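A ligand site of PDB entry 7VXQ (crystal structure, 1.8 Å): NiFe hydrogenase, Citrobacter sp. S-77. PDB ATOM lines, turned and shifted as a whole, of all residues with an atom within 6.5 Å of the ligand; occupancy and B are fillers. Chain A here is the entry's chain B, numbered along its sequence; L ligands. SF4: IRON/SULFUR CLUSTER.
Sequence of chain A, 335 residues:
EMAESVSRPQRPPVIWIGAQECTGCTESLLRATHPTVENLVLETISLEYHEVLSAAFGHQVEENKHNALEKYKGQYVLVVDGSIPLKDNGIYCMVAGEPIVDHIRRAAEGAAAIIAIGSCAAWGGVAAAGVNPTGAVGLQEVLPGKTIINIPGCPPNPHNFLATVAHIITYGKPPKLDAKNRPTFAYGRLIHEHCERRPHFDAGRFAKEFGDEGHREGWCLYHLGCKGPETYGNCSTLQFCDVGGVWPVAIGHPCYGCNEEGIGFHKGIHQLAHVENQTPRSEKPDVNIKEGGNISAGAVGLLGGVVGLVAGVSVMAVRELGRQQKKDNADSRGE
The backbone NH of Tyr 222 sits close to the side-chain sulfur of Cys 220 (3.3 Å).
N of Cys 226 lies within hydrogen-bond range of O of Leu 221, 3.3 Å away.
The guanidinium group of Arg 197 lies within hydrogen-bond range of the backbone carbonyl oxygen of Trp 219 (2.9 Å).
SG of Cys 226 sits close to N of Gly 228, at 3.5 Å.
The backbone carbonyl oxygen of Gly 228 sits at hydrogen-bond distance from the backbone NH of His 192 (3.2 Å).
NH1 of Arg 198 is in salt-bridge range of OE2 of Glu 193 (2.7 Å).
SG of Cys 226 sits close to N of Cys 255, 3.7 Å away.
The guanidinium group (NH1) of Arg 198 sits at hydrogen-bond distance from the backbone carbonyl oxygen (O) of His 192 (3.1 Å).
N of Arg 198 sits close to S4 of the ligand (3.5 Å).
The backbone NH (N) of Leu 221 sits close to a sulfur (S3) of the ligand (3.6 Å).
FE3 of the ligand is bound by ND1 of His 192, at 2.2 Å.
An iron atom (FE2) of the ligand is bound by the side-chain sulfur of Cys 195 (2.3 Å).
SG of Cys 226 is bound to FE4 of the ligand (2.3 Å).
An iron atom (FE1) of the ligand is bound by the side-chain sulfur (SG) of Cys 220 (2.3 Å).
Merely in contact with the ligand: Gly 228, Tyr 222, Arg 197, Val 249, Pro 229 and Phe 201.
Within 4 Å of the ligand: His 192, Cys 195, Arg 197, Arg 198, Phe 201, Cys 220, Leu 221, Tyr 222, Cys 226, Gly 228, Pro 229 and Val 249.
The nearest printed residue that does not touch the ligand is Ile 191 (4.1 Å).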
ATOM      1  N   ILE A 191       0.165   3.363  -6.962  1.00  0.00           N
ATOM      2  CA  ILE A 191       0.738   4.583  -6.345  1.00  0.00           C
ATOM      3  C   ILE A 191       0.059   4.789  -4.973  1.00  0.00           C
ATOM      4  O   ILE A 191       0.782   4.983  -3.989  1.00  0.00           O
ATOM      5  CB  ILE A 191       0.609   5.773  -7.322  1.00  0.00           C
ATOM      6  CG1 ILE A 191       1.548   5.596  -8.529  1.00  0.00           C
ATOM      7  CG2 ILE A 191       0.876   7.098  -6.615  1.00  0.00           C
ATOM      8  CD1 ILE A 191       1.228   6.568  -9.659  1.00  0.00           C
ATOM      9  N   HIS A 192      -1.265   4.655  -4.910  1.00  0.00           N
ATOM     10  CA  HIS A 192      -2.075   4.792  -3.669  1.00  0.00           C
ATOM     11  C   HIS A 192      -1.700   3.739  -2.606  1.00  0.00           C
ATOM     12  O   HIS A 192      -2.005   3.991  -1.436  1.00  0.00           O
ATOM     13  CB  HIS A 192      -3.566   4.669  -4.045  1.00  0.00           C
ATOM     14  CG  HIS A 192      -4.544   4.825  -2.942  1.00  0.00           C
ATOM     15  ND1 HIS A 192      -4.871   6.063  -2.440  1.00  0.00           N
ATOM     16  CD2 HIS A 192      -5.311   3.929  -2.271  1.00  0.00           C
ATOM     17  CE1 HIS A 192      -5.751   5.929  -1.466  1.00  0.00           C
ATOM     18  NE2 HIS A 192      -6.040   4.622  -1.346  1.00  0.00           N
ATOM     19  N   GLU A 193      -1.122   2.603  -2.970  1.00  0.00           N
ATOM     20  CA  GLU A 193      -0.702   1.587  -1.956  1.00  0.00           C
ATOM     21  C   GLU A 193       0.739   1.886  -1.493  1.00  0.00           C
ATOM     22  O   GLU A 193       1.300   1.080  -0.694  1.00  0.00           O
ATOM     23  CB  GLU A 193      -0.919   0.149  -2.470  1.00  0.00           C
ATOM     24  CG  GLU A 193      -2.409  -0.270  -2.516  1.00  0.00           C
ATOM     25  CD  GLU A 193      -3.195  -0.061  -1.220  1.00  0.00           C
ATOM     26  OE1 GLU A 193      -2.795  -0.665  -0.182  1.00  0.00           O
ATOM     27  OE2 GLU A 193      -4.121   0.790  -1.205  1.00  0.00           O
ATOM     28  N   CYS A 195       1.726   5.700  -1.050  1.00  0.00           N
ATOM     29  CA  CYS A 195       1.655   7.164  -1.131  1.00  0.00           C
ATOM     30  C   CYS A 195       1.678   7.797   0.246  1.00  0.00           C
ATOM     31  O   CYS A 195       0.912   7.378   1.106  1.00  0.00           O
ATOM     32  CB  CYS A 195       0.406   7.609  -1.876  1.00  0.00           C
ATOM     33  SG  CYS A 195       0.241   9.399  -1.916  1.00  0.00           S
ATOM     34  N   GLU A 196       2.509   8.839   0.424  1.00  0.00           N
ATOM     35  CA  GLU A 196       2.765   9.434   1.740  1.00  0.00           C
ATOM     36  C   GLU A 196       1.537  10.228   2.219  1.00  0.00           C
ATOM     37  O   GLU A 196       1.589  10.659   3.378  1.00  0.00           O
ATOM     38  CB  GLU A 196       3.985  10.348   1.642  1.00  0.00           C
ATOM     39  CG  GLU A 196       3.784  11.503   0.683  1.00  0.00           C
ATOM     40  CD  GLU A 196       4.309  11.339  -0.746  1.00  0.00           C
ATOM     41  OE1 GLU A 196       4.391  10.136  -1.258  1.00  0.00           O
ATOM     42  OE2 GLU A 196       4.645  12.422  -1.339  1.00  0.00           O
ATOM     43  N   ARG A 197       0.533  10.477   1.363  1.00  0.00           N
ATOM     44  CA  ARG A 197      -0.682  11.213   1.772  1.00  0.00           C
ATOM     45  C   ARG A 197      -1.769  10.239   2.236  1.00  0.00           C
ATOM     46  O   ARG A 197      -2.834  10.708   2.592  1.00  0.00           O
ATOM     47  CB  ARG A 197      -1.150  12.174   0.669  1.00  0.00           C
ATOM     48  CG  ARG A 197      -0.044  13.183   0.348  1.00  0.00           C
ATOM     49  CD  ARG A 197      -0.479  14.322  -0.486  1.00  0.00           C
ATOM     50  NE  ARG A 197       0.650  15.235  -0.655  1.00  0.00           N
ATOM     51  CZ  ARG A 197       0.519  16.515  -0.952  1.00  0.00           C
ATOM     52  NH1 ARG A 197      -0.674  17.037  -1.158  1.00  0.00           N
ATOM     53  NH2 ARG A 197       1.590  17.266  -1.132  1.00  0.00           N
ATOM     54  N   ARG A 198      -1.506   8.944   2.189  1.00  0.00           N
ATOM     55  CA  ARG A 198      -2.496   7.919   2.614  1.00  0.00           C
ATOM     56  C   ARG A 198      -3.053   8.203   4.013  1.00  0.00           C
ATOM     57  O   ARG A 198      -4.245   7.988   4.238  1.00  0.00           O
ATOM     58  CB  ARG A 198      -1.916   6.510   2.492  1.00  0.00           C
ATOM     59  CG  ARG A 198      -2.920   5.402   2.835  1.00  0.00           C
ATOM     60  CD  ARG A 198      -4.177   5.404   1.937  1.00  0.00           C
ATOM     61  NE  ARG A 198      -4.883   4.185   2.289  1.00  0.00           N
ATOM     62  CZ  ARG A 198      -4.759   3.004   1.696  1.00  0.00           C
ATOM     63  NH1 ARG A 198      -4.013   2.825   0.610  1.00  0.00           N
ATOM     64  NH2 ARG A 198      -5.397   1.979   2.238  1.00  0.00           N
ATOM     65  N   PRO A 199      -2.266   8.673   4.997  1.00  0.00           N
ATOM     66  CA  PRO A 199      -2.814   9.007   6.308  1.00  0.00           C
ATOM     67  C   PRO A 199      -3.918  10.073   6.279  1.00  0.00           C
ATOM     68  O   PRO A 199      -4.851  10.049   7.114  1.00  0.00           O
ATOM     69  CB  PRO A 199      -1.622   9.595   7.068  1.00  0.00           C
ATOM     70  CG  PRO A 199      -0.422   8.961   6.408  1.00  0.00           C
ATOM     71  CD  PRO A 199      -0.804   8.874   4.945  1.00  0.00           C
ATOM     72  N   PHE A 201      -5.869  10.615   3.576  1.00  0.00           N
ATOM     73  CA  PHE A 201      -6.961   9.889   2.893  1.00  0.00           C
ATOM     74  C   PHE A 201      -7.744   9.111   3.959  1.00  0.00           C
ATOM     75  O   PHE A 201      -8.984   9.158   3.970  1.00  0.00           O
ATOM     76  CB  PHE A 201      -6.389   8.917   1.855  1.00  0.00           C
ATOM     77  CG  PHE A 201      -7.386   8.073   1.111  1.00  0.00           C
ATOM     78  CD1 PHE A 201      -7.970   8.510  -0.072  1.00  0.00           C
ATOM     79  CD2 PHE A 201      -7.763   6.824   1.600  1.00  0.00           C
ATOM     80  CE1 PHE A 201      -8.893   7.728  -0.748  1.00  0.00           C
ATOM     81  CE2 PHE A 201      -8.670   6.053   0.918  1.00  0.00           C
ATOM     82  CZ  PHE A 201      -9.244   6.503  -0.247  1.00  0.00           C
ATOM     83  N   PHE A 206      -8.770  16.197   3.096  1.00  0.00           N
ATOM     84  CA  PHE A 206      -8.763  16.296   1.619  1.00  0.00           C
ATOM     85  C   PHE A 206      -8.609  17.740   1.200  1.00  0.00           C
ATOM     86  O   PHE A 206      -9.196  18.642   1.813  1.00  0.00           O
ATOM     87  CB  PHE A 206     -10.030  15.684   1.018  1.00  0.00           C
ATOM     88  CG  PHE A 206     -10.155  14.199   1.146  1.00  0.00           C
ATOM     89  CD1 PHE A 206      -9.264  13.335   0.531  1.00  0.00           C
ATOM     90  CD2 PHE A 206     -11.180  13.622   1.881  1.00  0.00           C
ATOM     91  CE1 PHE A 206      -9.403  11.967   0.632  1.00  0.00           C
ATOM     92  CE2 PHE A 206     -11.316  12.254   1.992  1.00  0.00           C
ATOM     93  CZ  PHE A 206     -10.454  11.416   1.346  1.00  0.00           C
ATOM     94  N   TRP A 219      -2.579  17.904   2.231  1.00  0.00           N
ATOM     95  CA  TRP A 219      -3.511  16.771   2.415  1.00  0.00           C
ATOM     96  C   TRP A 219      -3.699  16.010   1.113  1.00  0.00           C
ATOM     97  O   TRP A 219      -3.186  16.469   0.064  1.00  0.00           O
ATOM     98  CB  TRP A 219      -4.842  17.247   3.018  1.00  0.00           C
ATOM     99  CG  TRP A 219      -4.761  17.790   4.414  1.00  0.00           C
ATOM    100  CD1 TRP A 219      -3.710  17.719   5.286  1.00  0.00           C
ATOM    101  CD2 TRP A 219      -5.826  18.429   5.138  1.00  0.00           C
ATOM    102  NE1 TRP A 219      -4.017  18.349   6.461  1.00  0.00           N
ATOM    103  CE2 TRP A 219      -5.319  18.781   6.405  1.00  0.00           C
ATOM    104  CE3 TRP A 219      -7.149  18.774   4.809  1.00  0.00           C
ATOM    105  CZ2 TRP A 219      -6.088  19.440   7.367  1.00  0.00           C
ATOM    106  CZ3 TRP A 219      -7.916  19.425   5.760  1.00  0.00           C
ATOM    107  CH2 TRP A 219      -7.383  19.763   7.005  1.00  0.00           C
ATOM    108  N   CYS A 220      -4.433  14.915   1.186  1.00  0.00           N
ATOM    109  CA  CYS A 220      -4.749  13.978   0.094  1.00  0.00           C
ATOM    110  C   CYS A 220      -5.492  14.690  -1.043  1.00  0.00           C
ATOM    111  O   CYS A 220      -6.319  15.590  -0.755  1.00  0.00           O
ATOM    112  CB  CYS A 220      -5.599  12.828   0.590  1.00  0.00           C
ATOM    113  SG  CYS A 220      -6.090  11.674  -0.715  1.00  0.00           S
ATOM    114  N   LEU A 221      -5.167  14.299  -2.276  1.00  0.00           N
ATOM    115  CA  LEU A 221      -5.679  14.957  -3.506  1.00  0.00           C
ATOM    116  C   LEU A 221      -6.791  14.109  -4.129  1.00  0.00           C
ATOM    117  O   LEU A 221      -7.173  14.403  -5.307  1.00  0.00           O
ATOM    118  CB  LEU A 221      -4.485  15.157  -4.475  1.00  0.00           C
ATOM    119  CG  LEU A 221      -3.323  15.976  -3.905  1.00  0.00           C
ATOM    120  CD1 LEU A 221      -2.275  16.344  -4.986  1.00  0.00           C
ATOM    121  CD2 LEU A 221      -3.764  17.277  -3.259  1.00  0.00           C
ATOM    122  N   TYR A 222      -7.319  13.095  -3.415  1.00  0.00           N
ATOM    123  CA  TYR A 222      -8.334  12.150  -3.991  1.00  0.00           C
ATOM    124  C   TYR A 222      -9.485  12.915  -4.642  1.00  0.00           C
ATOM    125  O   TYR A 222      -9.891  12.566  -5.776  1.00  0.00           O
ATOM    126  CB  TYR A 222      -8.893  11.143  -2.952  1.00  0.00           C
ATOM    127  CG  TYR A 222      -9.917  10.227  -3.568  1.00  0.00           C
ATOM    128  CD1 TYR A 222      -9.536   9.172  -4.391  1.00  0.00           C
ATOM    129  CD2 TYR A 222     -11.274  10.445  -3.422  1.00  0.00           C
ATOM    130  CE1 TYR A 222     -10.471   8.359  -5.019  1.00  0.00           C
ATOM    131  CE2 TYR A 222     -12.218   9.635  -4.036  1.00  0.00           C
ATOM    132  CZ  TYR A 222     -11.822   8.580  -4.822  1.00  0.00           C
ATOM    133  OH  TYR A 222     -12.760   7.829  -5.513  1.00  0.00           O
ATOM    134  N   HIS A 223     -10.035  13.896  -3.924  1.00  0.00           N
ATOM    135  CA  HIS A 223     -11.244  14.677  -4.303  1.00  0.00           C
ATOM    136  C   HIS A 223     -10.908  15.774  -5.328  1.00  0.00           C
ATOM    137  O   HIS A 223     -11.842  16.389  -5.819  1.00  0.00           O
ATOM    138  CB  HIS A 223     -11.986  15.226  -3.074  1.00  0.00           C
ATOM    139  CG  HIS A 223     -12.759  14.137  -2.403  1.00  0.00           C
ATOM    140  ND1 HIS A 223     -13.883  13.569  -2.985  1.00  0.00           N
ATOM    141  CD2 HIS A 223     -12.523  13.444  -1.257  1.00  0.00           C
ATOM    142  CE1 HIS A 223     -14.313  12.575  -2.213  1.00  0.00           C
ATOM    143  NE2 HIS A 223     -13.482  12.461  -1.168  1.00  0.00           N
ATOM    144  N   CYS A 226      -7.308  12.620  -8.055  1.00  0.00           N
ATOM    145  CA  CYS A 226      -6.094  11.771  -8.013  1.00  0.00           C
ATOM    146  C   CYS A 226      -6.399  10.340  -8.481  1.00  0.00           C
ATOM    147  O   CYS A 226      -7.330   9.648  -7.968  1.00  0.00           O
ATOM    148  CB  CYS A 226      -5.456  11.806  -6.641  1.00  0.00           C
ATOM    149  SG  CYS A 226      -3.862  10.950  -6.621  1.00  0.00           S
ATOM    150  N   LYS A 227      -5.607   9.871  -9.439  1.00  0.00           N
ATOM    151  CA  LYS A 227      -5.764   8.543 -10.061  1.00  0.00           C
ATOM    152  C   LYS A 227      -4.831   7.519  -9.414  1.00  0.00           C
ATOM    153  O   LYS A 227      -4.744   6.394  -9.937  1.00  0.00           O
ATOM    154  CB  LYS A 227      -5.535   8.652 -11.573  1.00  0.00           C
ATOM    155  CG  LYS A 227      -6.544   9.544 -12.256  1.00  0.00           C
ATOM    156  CD  LYS A 227      -8.010   9.231 -11.858  1.00  0.00           C
ATOM    157  CE  LYS A 227      -9.015   9.949 -12.740  1.00  0.00           C
ATOM    158  NZ  LYS A 227      -8.838  11.402 -12.662  1.00  0.00           N
ATOM    159  N   GLY A 228      -4.137   7.905  -8.361  1.00  0.00           N
ATOM    160  CA  GLY A 228      -3.198   7.044  -7.638  1.00  0.00           C
ATOM    161  C   GLY A 228      -3.901   5.739  -7.267  1.00  0.00           C
ATOM    162  O   GLY A 228      -3.301   4.687  -7.392  1.00  0.00           O
ATOM    163  N   PRO A 229      -5.193   5.721  -6.881  1.00  0.00           N
ATOM    164  CA  PRO A 229      -5.839   4.437  -6.555  1.00  0.00           C
ATOM    165  C   PRO A 229      -5.981   3.425  -7.696  1.00  0.00           C
ATOM    166  O   PRO A 229      -6.256   2.248  -7.440  1.00  0.00           O
ATOM    167  CB  PRO A 229      -7.216   4.887  -6.053  1.00  0.00           C
ATOM    168  CG  PRO A 229      -6.974   6.244  -5.485  1.00  0.00           C
ATOM    169  CD  PRO A 229      -6.031   6.868  -6.510  1.00  0.00           C
ATOM    170  N   TRP A 247       7.302  14.758  -7.343  1.00  0.00           N
ATOM    171  CA  TRP A 247       6.312  14.064  -8.196  1.00  0.00           C
ATOM    172  C   TRP A 247       5.058  14.925  -8.190  1.00  0.00           C
ATOM    173  O   TRP A 247       4.959  15.888  -7.427  1.00  0.00           O
ATOM    174  CB  TRP A 247       6.134  12.604  -7.767  1.00  0.00           C
ATOM    175  CG  TRP A 247       5.443  12.359  -6.472  1.00  0.00           C
ATOM    176  CD1 TRP A 247       5.888  12.629  -5.214  1.00  0.00           C
ATOM    177  CD2 TRP A 247       4.190  11.651  -6.326  1.00  0.00           C
ATOM    178  NE1 TRP A 247       4.988  12.162  -4.290  1.00  0.00           N
ATOM    179  CE2 TRP A 247       3.949  11.551  -4.928  1.00  0.00           C
ATOM    180  CE3 TRP A 247       3.258  11.108  -7.221  1.00  0.00           C
ATOM    181  CZ2 TRP A 247       2.812  10.917  -4.418  1.00  0.00           C
ATOM    182  CZ3 TRP A 247       2.139  10.499  -6.718  1.00  0.00           C
ATOM    183  CH2 TRP A 247       1.929  10.385  -5.333  1.00  0.00           C
ATOM    184  N   VAL A 249       1.901  14.734  -7.201  1.00  0.00           N
ATOM    185  CA  VAL A 249       1.169  14.881  -5.906  1.00  0.00           C
ATOM    186  C   VAL A 249       1.976  15.702  -4.903  1.00  0.00           C
ATOM    187  O   VAL A 249       1.376  16.643  -4.286  1.00  0.00           O
ATOM    188  CB  VAL A 249       0.743  13.516  -5.356  1.00  0.00           C
ATOM    189  CG1 VAL A 249       0.357  13.660  -3.897  1.00  0.00           C
ATOM    190  CG2 VAL A 249      -0.355  12.938  -6.217  1.00  0.00           C
ATOM    191  N   PRO A 254      -3.140  16.335  -8.528  1.00  0.00           N
ATOM    192  CA  PRO A 254      -3.495  14.917  -8.545  1.00  0.00           C
ATOM    193  C   PRO A 254      -2.707  14.144  -9.624  1.00  0.00           C
ATOM    194  O   PRO A 254      -2.373  14.736 -10.632  1.00  0.00           O
ATOM    195  CB  PRO A 254      -5.007  14.935  -8.824  1.00  0.00           C
ATOM    196  CG  PRO A 254      -5.276  16.289  -9.410  1.00  0.00           C
ATOM    197  CD  PRO A 254      -4.286  17.231  -8.737  1.00  0.00           C
ATOM    198  N   CYS A 255      -2.425  12.863  -9.398  1.00  0.00           N
ATOM    199  CA  CYS A 255      -2.058  11.891 -10.440  1.00  0.00           C
ATOM    200  C   CYS A 255      -3.198  11.889 -11.471  1.00  0.00           C
ATOM    201  O   CYS A 255      -4.397  11.825 -11.058  1.00  0.00           O
ATOM    202  CB  CYS A 255      -1.766  10.517  -9.865  1.00  0.00           C
ATOM    203  SG  CYS A 255      -1.498   9.164 -11.045  1.00  0.00           S
HETATM  204 FE1  SF4 L   1      -4.496  10.477  -1.852  1.00  0.00          FE
HETATM  205 FE2  SF4 L   1      -2.003   9.645  -2.460  1.00  0.00          FE
HETATM  206 FE3  SF4 L   1      -4.110   8.097  -2.781  1.00  0.00          FE
HETATM  207 FE4  SF4 L   1      -3.667  10.175  -4.481  1.00  0.00          FE
HETATM  208  S1  SF4 L   1      -2.342   8.355  -4.334  1.00  0.00           S
HETATM  209  S2  SF4 L   1      -5.657   9.478  -3.555  1.00  0.00           S
HETATM  210  S3  SF4 L   1      -2.871  11.682  -3.012  1.00  0.00           S
HETATM  211  S4  SF4 L   1      -3.396   8.832  -0.795  1.00  0.00           S
